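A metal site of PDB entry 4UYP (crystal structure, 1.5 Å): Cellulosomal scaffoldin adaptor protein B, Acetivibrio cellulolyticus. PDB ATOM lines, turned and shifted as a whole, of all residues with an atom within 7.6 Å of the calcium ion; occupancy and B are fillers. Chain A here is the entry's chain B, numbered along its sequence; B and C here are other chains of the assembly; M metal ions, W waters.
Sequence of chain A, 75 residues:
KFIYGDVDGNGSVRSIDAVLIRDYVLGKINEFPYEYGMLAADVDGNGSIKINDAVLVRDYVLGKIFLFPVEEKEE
OD1 of Asp 53 lies close to N of Val 43 of chain A, at 3.3 Å.
OD2 of Asp 42 sits at hydrogen-bond distance from N of Gly 47, at 2.7 Å.
The side-chain carboxylate of Asp 42 sits close to the backbone NH of Gly 45.
N of Lys 50 lies close to OD2 of Asp 53 (2.9 Å).
NE2 of Gln 43 of chain C lies within hydrogen-bond range of OG of Ser 48 (2.9 Å).
The side-chain carboxylate (OD2) of Asp 44 is in hydrogen-bond range of the side-chain amide nitrogen (ND2) of Asn 52 (3.0 Å).
The backbone carbonyl oxygen (O) of Asn 46 sits close to the side-chain amide oxygen (OE1) of Gln 43 of chain C.
Five residues have an atom within 4 Å of the calcium ion: Asp 42, Asp 44, Asn 46, Ser 48 and Asp 53.
Along chain A the residues within 4 Å of the calcium ion span positions 42 to 53.
The calcium ion is bound by OD1 of Asp 42, O of Ser 48, OD1 of Asp 44, OD2 of Asp 53, OD1 of Asn 46, water W1 and OD1 of Asp 53.
The calcium ion has seven donor atoms within binding distance.
Water W1 lies within hydrogen-bond range of the side-chain amide oxygen (OD1) of Asn 52 (2.7 Å), the side-chain carboxylate (OD2) of Asp 44 (2.9 Å) and the side-chain amide nitrogen (ND2) of Asn 46 (3.1 Å).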
ATOM      1  N   ALA A  41      25.277  11.514 -19.380  1.00  0.00           N
ATOM      2  CA  ALA A  41      26.293  11.498 -20.469  1.00  0.00           C
ATOM      3  C   ALA A  41      26.415  12.856 -21.153  1.00  0.00           C
ATOM      4  O   ALA A  41      27.414  13.146 -21.797  1.00  0.00           O
ATOM      5  CB  ALA A  41      25.850  10.472 -21.523  1.00  0.00           C
ATOM      6  N   ASP A  42      25.369  13.683 -21.153  1.00  0.00           N
ATOM      7  CA  ASP A  42      25.347  14.890 -21.912  1.00  0.00           C
ATOM      8  C   ASP A  42      26.058  16.023 -21.094  1.00  0.00           C
ATOM      9  O   ASP A  42      25.380  16.995 -20.637  1.00  0.00           O
ATOM     10  CB  ASP A  42      23.884  15.303 -22.335  1.00  0.00           C
ATOM     11  CG  ASP A  42      23.867  16.540 -23.134  1.00  0.00           C
ATOM     12  OD1 ASP A  42      24.882  16.924 -23.822  1.00  0.00           O
ATOM     13  OD2 ASP A  42      22.811  17.221 -23.159  1.00  0.00           O
ATOM     14  N   VAL A  43      27.362  15.903 -20.974  1.00  0.00           N
ATOM     15  CA  VAL A  43      28.074  16.776 -20.059  1.00  0.00           C
ATOM     16  C   VAL A  43      28.262  18.152 -20.654  1.00  0.00           C
ATOM     17  O   VAL A  43      28.633  19.081 -19.878  1.00  0.00           O
ATOM     18  CB  VAL A  43      29.363  16.142 -19.566  1.00  0.00           C
ATOM     19  CG1 VAL A  43      29.103  14.913 -18.744  1.00  0.00           C
ATOM     20  CG2 VAL A  43      30.274  15.689 -20.725  1.00  0.00           C
ATOM     21  N   ASP A  44      28.136  18.403 -21.965  1.00  0.00           N
ATOM     22  CA  ASP A  44      28.087  19.789 -22.442  1.00  0.00           C
ATOM     23  C   ASP A  44      26.659  20.424 -22.413  1.00  0.00           C
ATOM     24  O   ASP A  44      26.521  21.613 -22.695  1.00  0.00           O
ATOM     25  CB  ASP A  44      28.869  19.968 -23.757  1.00  0.00           C
ATOM     26  CG  ASP A  44      28.105  19.444 -25.029  1.00  0.00           C
ATOM     27  OD1 ASP A  44      27.019  18.838 -24.802  1.00  0.00           O
ATOM     28  OD2 ASP A  44      28.601  19.842 -26.102  1.00  0.00           O
ATOM     29  N   GLY A  45      25.692  19.676 -22.046  1.00  0.00           N
ATOM     30  CA  GLY A  45      24.339  20.127 -21.820  1.00  0.00           C
ATOM     31  C   GLY A  45      23.656  20.578 -23.087  1.00  0.00           C
ATOM     32  O   GLY A  45      22.681  21.322 -23.033  1.00  0.00           O
ATOM     33  N   ASN A  46      24.129  20.108 -24.254  1.00  0.00           N
ATOM     34  CA  ASN A  46      23.505  20.583 -25.514  1.00  0.00           C
ATOM     35  C   ASN A  46      22.328  19.816 -25.955  1.00  0.00           C
ATOM     36  O   ASN A  46      21.637  20.276 -26.926  1.00  0.00           O
ATOM     37  CB  ASN A  46      24.557  20.723 -26.634  1.00  0.00           C
ATOM     38  CG  ASN A  46      24.983  19.377 -27.222  1.00  0.00           C
ATOM     39  OD1 ASN A  46      24.781  18.327 -26.674  1.00  0.00           O
ATOM     40  ND2 ASN A  46      25.578  19.468 -28.350  1.00  0.00           N
ATOM     41  N   GLY A  47      21.970  18.722 -25.291  1.00  0.00           N
ATOM     42  CA  GLY A  47      20.807  17.951 -25.618  1.00  0.00           C
ATOM     43  C   GLY A  47      20.997  16.717 -26.461  1.00  0.00           C
ATOM     44  O   GLY A  47      20.078  15.906 -26.587  1.00  0.00           O
ATOM     45  N   SER A  48      22.262  16.501 -26.909  1.00  0.00           N
ATOM     46  CA  SER A  48      22.612  15.335 -27.719  1.00  0.00           C
ATOM     47  C   SER A  48      23.846  14.710 -27.133  1.00  0.00           C
ATOM     48  O   SER A  48      24.697  15.405 -26.522  1.00  0.00           O
ATOM     49  CB  SER A  48      22.927  15.636 -29.162  1.00  0.00           C
ATOM     50  OG  SER A  48      21.751  16.071 -29.878  1.00  0.00           O
ATOM     51  N   ILE A  49      23.944  13.377 -27.270  1.00  0.00           N
ATOM     52  CA  ILE A  49      25.165  12.671 -26.905  1.00  0.00           C
ATOM     53  C   ILE A  49      26.068  12.602 -28.163  1.00  0.00           C
ATOM     54  O   ILE A  49      25.644  12.084 -29.215  1.00  0.00           O
ATOM     55  CB  ILE A  49      24.826  11.317 -26.358  1.00  0.00           C
ATOM     56  CG1 ILE A  49      23.728  11.439 -25.276  1.00  0.00           C
ATOM     57  CG2 ILE A  49      26.036  10.613 -25.746  1.00  0.00           C
ATOM     58  CD1 ILE A  49      23.447  10.131 -24.544  1.00  0.00           C
ATOM     59  N   LYS A  50      27.259  13.163 -28.070  1.00  0.00           N
ATOM     60  CA  LYS A  50      28.202  13.219 -29.188  1.00  0.00           C
ATOM     61  C   LYS A  50      29.543  12.909 -28.692  1.00  0.00           C
ATOM     62  O   LYS A  50      29.825  12.753 -27.506  1.00  0.00           O
ATOM     63  CB  LYS A  50      28.192  14.566 -29.847  1.00  0.00           C
ATOM     64  CG  LYS A  50      26.787  15.036 -30.349  1.00  0.00           C
ATOM     65  CD  LYS A  50      26.823  16.420 -30.928  1.00  0.00           C
ATOM     66  CE  LYS A  50      27.546  16.469 -32.218  1.00  0.00           C
ATOM     67  NZ  LYS A  50      27.483  17.840 -32.849  1.00  0.00           N
ATOM     68  N   ILE A  51      30.515  12.715 -29.644  1.00  0.00           N
ATOM     69  CA  ILE A  51      31.835  12.298 -29.226  1.00  0.00           C
ATOM     70  C   ILE A  51      32.488  13.268 -28.235  1.00  0.00           C
ATOM     71  O   ILE A  51      33.327  12.804 -27.440  1.00  0.00           O
ATOM     72  CB  ILE A  51      32.756  12.003 -30.510  1.00  0.00           C
ATOM     73  CG1 ILE A  51      34.065  11.218 -30.141  1.00  0.00           C
ATOM     74  CG2 ILE A  51      33.090  13.285 -31.234  1.00  0.00           C
ATOM     75  CD1 ILE A  51      33.801   9.911 -29.422  1.00  0.00           C
ATOM     76  N   ASN A  52      32.185  14.566 -28.359  1.00  0.00           N
ATOM     77  CA  ASN A  52      32.905  15.419 -27.413  1.00  0.00           C
ATOM     78  C   ASN A  52      32.412  15.223 -25.992  1.00  0.00           C
ATOM     79  O   ASN A  52      33.216  15.475 -25.079  1.00  0.00           O
ATOM     80  CB  ASN A  52      32.698  16.880 -27.815  1.00  0.00           C
ATOM     81  CG  ASN A  52      31.280  17.361 -27.589  1.00  0.00           C
ATOM     82  OD1 ASN A  52      30.287  16.717 -27.988  1.00  0.00           O
ATOM     83  ND2 ASN A  52      31.135  18.529 -26.910  1.00  0.00           N
ATOM     84  N   ASP A  53      31.204  14.726 -25.766  1.00  0.00           N
ATOM     85  CA  ASP A  53      30.795  14.382 -24.378  1.00  0.00           C
ATOM     86  C   ASP A  53      31.705  13.343 -23.846  1.00  0.00           C
ATOM     87  O   ASP A  53      32.098  13.363 -22.685  1.00  0.00           O
ATOM     88  CB  ASP A  53      29.347  13.925 -24.346  1.00  0.00           C
ATOM     89  CG  ASP A  53      28.366  14.973 -24.748  1.00  0.00           C
ATOM     90  OD1 ASP A  53      28.260  16.061 -24.116  1.00  0.00           O
ATOM     91  OD2 ASP A  53      27.532  14.773 -25.710  1.00  0.00           O
ATOM     92  N   ALA A  54      32.112  12.327 -24.704  1.00  0.00           N
ATOM     93  CA  ALA A  54      32.956  11.265 -24.186  1.00  0.00           C
ATOM     94  C   ALA A  54      34.356  11.847 -23.822  1.00  0.00           C
ATOM     95  O   ALA A  54      34.882  11.463 -22.785  1.00  0.00           O
ATOM     96  CB  ALA A  54      33.078  10.178 -25.333  1.00  0.00           C
ATOM     97  N   LEU A  56      35.079  14.875 -23.021  1.00  0.00           N
ATOM     98  CA  LEU A  56      34.943  15.691 -21.790  1.00  0.00           C
ATOM     99  C   LEU A  56      34.953  14.856 -20.574  1.00  0.00           C
ATOM    100  O   LEU A  56      35.622  15.232 -19.565  1.00  0.00           O
ATOM    101  CB  LEU A  56      33.702  16.579 -21.902  1.00  0.00           C
ATOM    102  CG  LEU A  56      33.790  17.779 -22.872  1.00  0.00           C
ATOM    103  CD1 LEU A  56      32.412  18.383 -23.122  1.00  0.00           C
ATOM    104  CD2 LEU A  56      34.742  18.909 -22.338  1.00  0.00           C
ATOM    105  N   TYR B 122      35.562  17.927 -33.864  1.00  0.00           N
ATOM    106  CA  TYR B 122      35.804  18.953 -32.770  1.00  0.00           C
ATOM    107  C   TYR B 122      37.258  19.410 -32.795  1.00  0.00           C
ATOM    108  O   TYR B 122      38.185  18.613 -32.829  1.00  0.00           O
ATOM    109  CB  TYR B 122      35.487  18.377 -31.429  1.00  0.00           C
ATOM    110  CG  TYR B 122      33.979  18.313 -31.164  1.00  0.00           C
ATOM    111  CD1 TYR B 122      33.169  17.282 -31.700  1.00  0.00           C
ATOM    112  CD2 TYR B 122      33.347  19.354 -30.474  1.00  0.00           C
ATOM    113  CE1 TYR B 122      31.807  17.321 -31.503  1.00  0.00           C
ATOM    114  CE2 TYR B 122      31.981  19.381 -30.337  1.00  0.00           C
ATOM    115  CZ  TYR B 122      31.216  18.360 -30.819  1.00  0.00           C
ATOM    116  OH  TYR B 122      29.822  18.368 -30.700  1.00  0.00           O
ATOM    117  N   GLN C  43      21.089  19.186 -33.251  1.00  0.00           N
ATOM    118  CA  GLN C  43      21.564  20.500 -32.658  1.00  0.00           C
ATOM    119  C   GLN C  43      21.669  21.593 -33.634  1.00  0.00           C
ATOM    120  O   GLN C  43      21.813  22.814 -33.235  1.00  0.00           O
ATOM    121  CB  GLN C  43      23.037  20.251 -32.196  1.00  0.00           C
ATOM    122  CG  GLN C  43      23.087  19.224 -31.097  1.00  0.00           C
ATOM    123  CD  GLN C  43      22.213  19.689 -30.015  1.00  0.00           C
ATOM    124  OE1 GLN C  43      22.485  20.842 -29.566  1.00  0.00           O
ATOM    125  NE2 GLN C  43      21.303  18.912 -29.479  1.00  0.00           N
HETATM  126 CA    CA M   1      26.294  16.784 -25.598  1.00  0.00          CA
HETATM  127  O   HOH W   1      27.732  17.443 -27.424  1.00  0.00           O
